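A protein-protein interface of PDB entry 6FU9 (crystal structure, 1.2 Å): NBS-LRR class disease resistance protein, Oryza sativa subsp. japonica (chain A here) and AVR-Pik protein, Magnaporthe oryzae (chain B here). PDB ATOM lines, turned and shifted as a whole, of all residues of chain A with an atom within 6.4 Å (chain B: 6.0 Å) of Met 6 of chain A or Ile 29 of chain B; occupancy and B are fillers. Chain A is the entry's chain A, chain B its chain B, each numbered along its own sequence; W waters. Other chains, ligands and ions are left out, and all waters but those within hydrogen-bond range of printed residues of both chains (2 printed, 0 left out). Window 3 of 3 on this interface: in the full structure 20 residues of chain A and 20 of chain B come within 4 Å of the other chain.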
ATOM      1  N   GLY A   4      16.588  28.355  10.467  1.00  0.00           N
ATOM      2  CA  GLY A   4      16.340  29.661   9.893  1.00  0.00           C
ATOM      3  C   GLY A   4      14.926  30.091  10.033  1.00  0.00           C
ATOM      4  O   GLY A   4      14.047  29.260  10.320  1.00  0.00           O
ATOM      5  N   GLU A   5      14.678  31.343   9.763  1.00  0.00           N
ATOM      6  CA  GLU A   5      13.280  31.789   9.583  1.00  0.00           C
ATOM      7  C   GLU A   5      12.607  30.958   8.503  1.00  0.00           C
ATOM      8  O   GLU A   5      13.157  30.759   7.435  1.00  0.00           O
ATOM      9  CB  GLU A   5      13.323  33.277   9.197  1.00  0.00           C
ATOM     10  CG  GLU A   5      11.981  33.956   9.157  1.00  0.00           C
ATOM     11  CD  GLU A   5      12.166  35.366   8.639  1.00  0.00           C
ATOM     12  OE1 GLU A   5      12.213  36.289   9.463  1.00  0.00           O
ATOM     13  OE2 GLU A   5      12.349  35.551   7.435  1.00  0.00           O
ATOM     14  N   MET A   6      11.393  30.492   8.816  1.00  0.00           N
ATOM     15  CA  MET A   6      10.715  29.569   7.919  1.00  0.00           C
ATOM     16  C   MET A   6      10.222  30.256   6.636  1.00  0.00           C
ATOM     17  O   MET A   6       9.971  31.426   6.597  1.00  0.00           O
ATOM     18  CB  MET A   6       9.561  28.938   8.671  1.00  0.00           C
ATOM     19  CG  MET A   6      10.088  27.960   9.728  1.00  0.00           C
ATOM     20  SD  MET A   6       8.901  27.217  10.811  1.00  0.00           S
ATOM     21  CE  MET A   6       8.266  26.301   9.511  1.00  0.00           C
ATOM     22  N   GLN A   7      10.107  29.406   5.622  1.00  0.00           N
ATOM     23  CA  GLN A   7       9.616  29.753   4.310  1.00  0.00           C
ATOM     24  C   GLN A   7       8.125  29.349   4.161  1.00  0.00           C
ATOM     25  O   GLN A   7       7.732  28.357   4.769  1.00  0.00           O
ATOM     26  CB  GLN A   7      10.318  28.847   3.247  1.00  0.00           C
ATOM     27  CG  GLN A   7      11.781  29.022   2.902  1.00  0.00           C
ATOM     28  CD  GLN A   7      12.257  27.754   2.199  1.00  0.00           C
ATOM     29  OE1 GLN A   7      12.489  26.752   2.773  1.00  0.00           O
ATOM     30  NE2 GLN A   7      12.530  27.898   0.916  1.00  0.00           N
ATOM     31  N   LYS A   8       7.414  30.075   3.338  1.00  0.00           N
ATOM     32  CA  LYS A   8       6.049  29.752   2.899  1.00  0.00           C
ATOM     33  C   LYS A   8       5.994  29.798   1.434  1.00  0.00           C
ATOM     34  O   LYS A   8       6.307  30.855   0.803  1.00  0.00           O
ATOM     35  CB  LYS A   8       5.062  30.731   3.509  1.00  0.00           C
ATOM     36  CG  LYS A   8       3.615  30.433   3.160  1.00  0.00           C
ATOM     37  CD  LYS A   8       2.690  31.395   3.917  1.00  0.00           C
ATOM     38  CE  LYS A   8       1.263  31.253   3.608  1.00  0.00           C
ATOM     39  NZ  LYS A   8       0.588  32.260   4.447  1.00  0.00           N
ATOM     40  N   GLY A  33      12.903  19.408   4.221  1.00  0.00           N
ATOM     41  CA  GLY A  33      12.651  20.773   4.658  1.00  0.00           C
ATOM     42  C   GLY A  33      11.191  21.063   4.975  1.00  0.00           C
ATOM     43  O   GLY A  33      10.916  22.125   5.564  1.00  0.00           O
ATOM     44  N   HIS A  35       7.802  21.215   6.793  1.00  0.00           N
ATOM     45  CA  HIS A  35       7.187  21.017   8.089  1.00  0.00           C
ATOM     46  C   HIS A  35       5.704  20.729   8.011  1.00  0.00           C
ATOM     47  O   HIS A  35       5.210  19.947   8.836  1.00  0.00           O
ATOM     48  CB  HIS A  35       7.400  22.241   8.951  1.00  0.00           C
ATOM     49  CG  HIS A  35       8.821  22.426   9.335  1.00  0.00           C
ATOM     50  ND1 HIS A  35       9.191  23.300  10.318  1.00  0.00           N
ATOM     51  CD2 HIS A  35       9.952  21.898   8.839  1.00  0.00           C
ATOM     52  CE1 HIS A  35      10.511  23.302  10.410  1.00  0.00           C
ATOM     53  NE2 HIS A  35      10.992  22.432   9.544  1.00  0.00           N
ATOM     54  N   SER A  36       4.997  21.357   7.103  1.00  0.00           N
ATOM     55  CA  SER A  36       3.549  21.152   6.953  1.00  0.00           C
ATOM     56  C   SER A  36       3.111  21.543   5.590  1.00  0.00           C
ATOM     57  O   SER A  36       3.735  22.400   4.918  1.00  0.00           O
ATOM     58  CB  SER A  36       2.813  21.814   8.057  1.00  0.00           C
ATOM     59  OG  SER A  36       3.022  23.164   8.067  1.00  0.00           O
ATOM     60  N   VAL A  50       4.958  24.970   4.169  1.00  0.00           N
ATOM     61  CA  VAL A  50       5.772  25.687   5.155  1.00  0.00           C
ATOM     62  C   VAL A  50       6.912  24.831   5.555  1.00  0.00           C
ATOM     63  O   VAL A  50       6.795  23.641   5.794  1.00  0.00           O
ATOM     64  CB  VAL A  50       4.910  26.074   6.377  1.00  0.00           C
ATOM     65  CG1 VAL A  50       5.693  26.586   7.517  1.00  0.00           C
ATOM     66  CG2 VAL A  50       3.830  27.100   5.937  1.00  0.00           C
ATOM     67  N   GLY A  51       8.098  25.432   5.710  1.00  0.00           N
ATOM     68  CA  GLY A  51       9.238  24.685   6.181  1.00  0.00           C
ATOM     69  C   GLY A  51      10.522  25.489   6.197  1.00  0.00           C
ATOM     70  O   GLY A  51      10.480  26.712   6.314  1.00  0.00           O
ATOM     71  N   ASP A  52      11.642  24.790   6.173  1.00  0.00           N
ATOM     72  CA  ASP A  52      12.943  25.422   6.322  1.00  0.00           C
ATOM     73  C   ASP A  52      13.943  24.691   5.452  1.00  0.00           C
ATOM     74  O   ASP A  52      14.205  23.540   5.629  1.00  0.00           O
ATOM     75  CB  ASP A  52      13.341  25.440   7.818  1.00  0.00           C
ATOM     76  CG  ASP A  52      14.751  26.029   8.082  1.00  0.00           C
ATOM     77  OD1 ASP A  52      15.237  26.871   7.290  1.00  0.00           O
ATOM     78  OD2 ASP A  52      15.325  25.688   9.141  1.00  0.00           O
ATOM     79  N   SER A  76       7.219  33.560   0.216  1.00  0.00           N
ATOM     80  CA  SER A  76       7.348  34.509   1.293  1.00  0.00           C
ATOM     81  C   SER A  76       8.059  33.842   2.472  1.00  0.00           C
ATOM     82  O   SER A  76       8.278  32.635   2.472  1.00  0.00           O
ATOM     83  CB  SER A  76       6.011  35.078   1.694  1.00  0.00           C
ATOM     84  OG  SER A  76       5.150  34.071   2.184  1.00  0.00           O
ATOM     85  N   GLN A  77       8.450  34.671   3.433  1.00  0.00           N
ATOM     86  CA  GLN A  77       8.984  34.200   4.681  1.00  0.00           C
ATOM     87  C   GLN A  77       7.889  34.264   5.739  1.00  0.00           C
ATOM     88  O   GLN A  77       7.001  35.098   5.662  1.00  0.00           O
ATOM     89  CB  GLN A  77      10.167  35.058   5.125  1.00  0.00           C
ATOM     90  CG  GLN A  77      11.444  34.837   4.261  1.00  0.00           C
ATOM     91  CD  GLN A  77      12.075  33.479   4.481  1.00  0.00           C
ATOM     92  OE1 GLN A  77      12.037  32.604   3.603  1.00  0.00           O
ATOM     93  NE2 GLN A  77      12.614  33.266   5.651  1.00  0.00           N
ATOM     94  N   VAL A  78       7.968  33.399   6.748  1.00  0.00           N
ATOM     95  CA  VAL A  78       7.055  33.438   7.861  1.00  0.00           C
ATOM     96  C   VAL A  78       7.453  34.594   8.808  1.00  0.00           C
ATOM     97  O   VAL A  78       8.654  34.749   9.082  1.00  0.00           O
ATOM     98  CB  VAL A  78       7.078  32.119   8.606  1.00  0.00           C
ATOM     99  CG1 VAL A  78       6.274  32.165   9.922  1.00  0.00           C
ATOM    100  CG2 VAL A  78       6.523  31.020   7.714  1.00  0.00           C
ATOM    101  N   LYS A  79       6.487  35.394   9.243  1.00  0.00           N
ATOM    102  CA  LYS A  79       6.716  36.411  10.252  1.00  0.00           C
ATOM    103  C   LYS A  79       6.716  35.752  11.629  1.00  0.00           C
ATOM    104  O   LYS A  79       5.649  35.350  12.150  1.00  0.00           O
ATOM    105  CB  LYS A  79       5.663  37.506  10.176  1.00  0.00           C
ATOM    106  CG  LYS A  79       5.957  38.661  11.127  1.00  0.00           C
ATOM    107  CD  LYS A  79       4.928  39.784  11.105  1.00  0.00           C
ATOM    108  CE  LYS A  79       3.614  39.346  11.738  1.00  0.00           C
ATOM    109  NZ  LYS A  79       2.654  40.489  11.830  1.00  0.00           N
ATOM    110  N   GLU A  80       7.910  35.570  12.196  1.00  0.00           N
ATOM    111  CA  GLU A  80       8.047  34.768  13.416  1.00  0.00           C
ATOM    112  C   GLU A  80       8.058  35.579  14.668  1.00  0.00           C
ATOM    113  O   GLU A  80       7.839  35.006  15.712  1.00  0.00           O
ATOM    114  CB  GLU A  80       9.363  33.980  13.368  1.00  0.00           C
ATOM    115  CG  GLU A  80       9.317  32.920  12.284  1.00  0.00           C
ATOM    116  CD  GLU A  80      10.536  32.052  12.210  1.00  0.00           C
ATOM    117  OE1 GLU A  80      11.619  32.425  12.746  1.00  0.00           O
ATOM    118  OE2 GLU A  80      10.464  30.998  11.535  1.00  0.00           O
ATOM    119  N   HIS B  26      -1.458  26.809   9.727  1.00  0.00           N
ATOM    120  CA  HIS B  26      -0.458  25.807  10.034  1.00  0.00           C
ATOM    121  C   HIS B  26      -0.028  25.907  11.497  1.00  0.00           C
ATOM    122  O   HIS B  26       0.170  26.978  12.032  1.00  0.00           O
ATOM    123  CB  HIS B  26       0.797  25.988   9.161  1.00  0.00           C
ATOM    124  CG  HIS B  26       0.567  25.867   7.696  1.00  0.00           C
ATOM    125  ND1 HIS B  26       0.918  24.751   6.965  1.00  0.00           N
ATOM    126  CD2 HIS B  26       0.009  26.741   6.824  1.00  0.00           C
ATOM    127  CE1 HIS B  26       0.490  24.907   5.741  1.00  0.00           C
ATOM    128  NE2 HIS B  26      -0.033  26.113   5.613  1.00  0.00           N
ATOM    129  N   PRO B  27       0.023  24.782  12.171  1.00  0.00           N
ATOM    130  CA  PRO B  27       0.162  24.825  13.624  1.00  0.00           C
ATOM    131  C   PRO B  27       1.526  25.296  14.123  1.00  0.00           C
ATOM    132  O   PRO B  27       1.615  25.781  15.268  1.00  0.00           O
ATOM    133  CB  PRO B  27      -0.101  23.376  14.039  1.00  0.00           C
ATOM    134  CG  PRO B  27       0.400  22.608  12.857  1.00  0.00           C
ATOM    135  CD  PRO B  27      -0.096  23.412  11.678  1.00  0.00           C
ATOM    136  N   GLY B  28       2.594  25.186  13.342  1.00  0.00           N
ATOM    137  CA  GLY B  28       3.911  25.475  13.964  1.00  0.00           C
ATOM    138  C   GLY B  28       4.405  26.901  13.795  1.00  0.00           C
ATOM    139  O   GLY B  28       5.551  27.199  14.132  1.00  0.00           O
ATOM    140  N   ILE B  29       3.556  27.775  13.273  1.00  0.00           N
ATOM    141  CA  ILE B  29       3.954  29.138  12.922  1.00  0.00           C
ATOM    142  C   ILE B  29       2.842  30.059  13.410  1.00  0.00           C
ATOM    143  O   ILE B  29       1.682  29.630  13.584  1.00  0.00           O
ATOM    144  CB  ILE B  29       4.203  29.340  11.404  1.00  0.00           C
ATOM    145  CG1 ILE B  29       2.953  28.968  10.553  1.00  0.00           C
ATOM    146  CG2 ILE B  29       5.443  28.592  10.933  1.00  0.00           C
ATOM    147  CD1 ILE B  29       3.130  29.361   9.105  1.00  0.00           C
ATOM    148  N   PRO B  30       3.126  31.337  13.573  1.00  0.00           N
ATOM    149  CA  PRO B  30       2.102  32.225  14.043  1.00  0.00           C
ATOM    150  C   PRO B  30       0.898  32.296  13.089  1.00  0.00           C
ATOM    151  O   PRO B  30       1.053  32.157  11.885  1.00  0.00           O
ATOM    152  CB  PRO B  30       2.850  33.582  14.172  1.00  0.00           C
ATOM    153  CG  PRO B  30       4.241  33.170  14.418  1.00  0.00           C
ATOM    154  CD  PRO B  30       4.435  32.001  13.497  1.00  0.00           C
ATOM    155  N   VAL B  31      -0.260  32.537  13.660  1.00  0.00           N
ATOM    156  CA  VAL B  31      -1.454  32.670  12.829  1.00  0.00           C
ATOM    157  C   VAL B  31      -1.386  33.983  12.068  1.00  0.00           C
ATOM    158  O   VAL B  31      -1.247  35.044  12.693  1.00  0.00           O
ATOM    159  CB  VAL B  31      -2.718  32.592  13.727  1.00  0.00           C
ATOM    160  CG1 VAL B  31      -3.959  32.827  12.870  1.00  0.00           C
ATOM    161  CG2 VAL B  31      -2.810  31.243  14.407  1.00  0.00           C
ATOM    162  N   PRO B  32      -1.534  33.951  10.740  1.00  0.00           N
ATOM    163  CA  PRO B  32      -1.477  35.227   9.989  1.00  0.00           C
ATOM    164  C   PRO B  32      -2.725  36.074  10.253  1.00  0.00           C
ATOM    165  O   PRO B  32      -3.840  35.575  10.380  1.00  0.00           O
ATOM    166  CB  PRO B  32      -1.386  34.751   8.520  1.00  0.00           C
ATOM    167  CG  PRO B  32      -2.028  33.390   8.555  1.00  0.00           C
ATOM    168  CD  PRO B  32      -1.588  32.808   9.865  1.00  0.00           C
ATOM    169  N   TYR B  51       0.443  37.654   6.560  1.00  0.00           N
ATOM    170  CA  TYR B  51       0.780  38.405   7.741  1.00  0.00           C
ATOM    171  C   TYR B  51       0.616  39.890   7.555  1.00  0.00           C
ATOM    172  O   TYR B  51       0.868  40.395   6.472  1.00  0.00           O
ATOM    173  CB  TYR B  51       2.242  38.108   8.182  1.00  0.00           C
ATOM    174  CG  TYR B  51       2.442  36.681   8.636  1.00  0.00           C
ATOM    175  CD1 TYR B  51       1.941  36.240   9.903  1.00  0.00           C
ATOM    176  CD2 TYR B  51       3.013  35.730   7.853  1.00  0.00           C
ATOM    177  CE1 TYR B  51       2.038  34.937  10.291  1.00  0.00           C
ATOM    178  CE2 TYR B  51       3.118  34.391   8.237  1.00  0.00           C
ATOM    179  CZ  TYR B  51       2.573  33.982   9.468  1.00  0.00           C
ATOM    180  OH  TYR B  51       2.641  32.672   9.795  1.00  0.00           O
HETATM  181  O   HOH W   1       4.003  24.193  10.438  1.00  0.00           O
HETATM  182  O   HOH W   2       0.991  31.634   7.349  1.00  0.00           O
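OG of Ser 36 of chain A lies within hydrogen-bond range of ND1 of His 26 of chain B, at 2.9 Å.
Printed residues of chain B that touch a printed residue of chain A: His 26, Ile 29, Pro 30 and Tyr 51. Printed residues of chain A that touch a printed residue of chain B: Met 6, Ser 36, Val 50, Val 78 and Lys 79. Hydrophobic or aromatic side chains of chain A that line the printed part of chain B: Met 6, Val 50 and Val 78. Among the printed residues, no Asp or Glu carboxylate lies within 4 Å of a Lys or Arg side-chain nitrogen of the other chain.
Met 6 of chain A touches Ile 29 of chain B. His 26 of chain B touches Val 50 of chain A (ND1 to CG2, 3.9 Å). Ile 29 of chain B touches Val 50 of chain A (CD1 to CG2, 3.95 Å). Ile 29 of chain B touches Val 78 of chain A. CG1 of Val 78 of chain A touches OH of Tyr 51 of chain B (3.7 Å). Pro 30 of chain B touches Lys 79 of chain A. Lys 79 of chain A touches Tyr 51 of chain B.
Water W1 lies within hydrogen-bond range of OG of Ser 36 of chain A (2.8 Å) and N of Gly 28 of chain B (3.4 Å). Water W2 lies within hydrogen-bond range of NZ of Lys 8 of chain A and OH of Tyr 51 of chain B.
NE2 of Gln 77 of chain A lies within hydrogen-bond range of O of Met 6 of chain A (3.4 Å). The backbone NH (N) of Val 78 of chain A sits at hydrogen-bond distance from the backbone carbonyl oxygen (O) of Met 6 of chain A, at 2.8 Å. The side-chain carboxylate (OE2) of Glu 80 of chain A sits at hydrogen-bond distance from the backbone NH (N) of Met 6 of chain A. N of His 35 of chain A is in hydrogen-bond range of O of Val 50 of chain A (2.8 Å). O of Ser 36 of chain A sits at hydrogen-bond distance from N of Val 50 of chain A (2.9 Å). The side-chain hydroxyl (OH) of Tyr 51 of chain B lies within hydrogen-bond range of the backbone carbonyl oxygen (O) of Pro 30 of chain B, 2.7 Å away.
Ile 29 of chain B touches just these residues of chain A: Met 6 (3.7 Å), Val 50 (3.95 Å) and Val 78 (3.8 Å). Of the printed residues of chain B, Lys 79 of chain A touches Pro 30 (3.4 Å) and Tyr 51 (3.7 Å). Printed residues of chain B within 4 Å of Val 50 of chain A: His 26 (3.9 Å) and Ile 29 (3.95 Å). The nearest printed residue of chain B that does not touch Val 78 of chain A is Pro 30 of chain B (4.02 Å).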
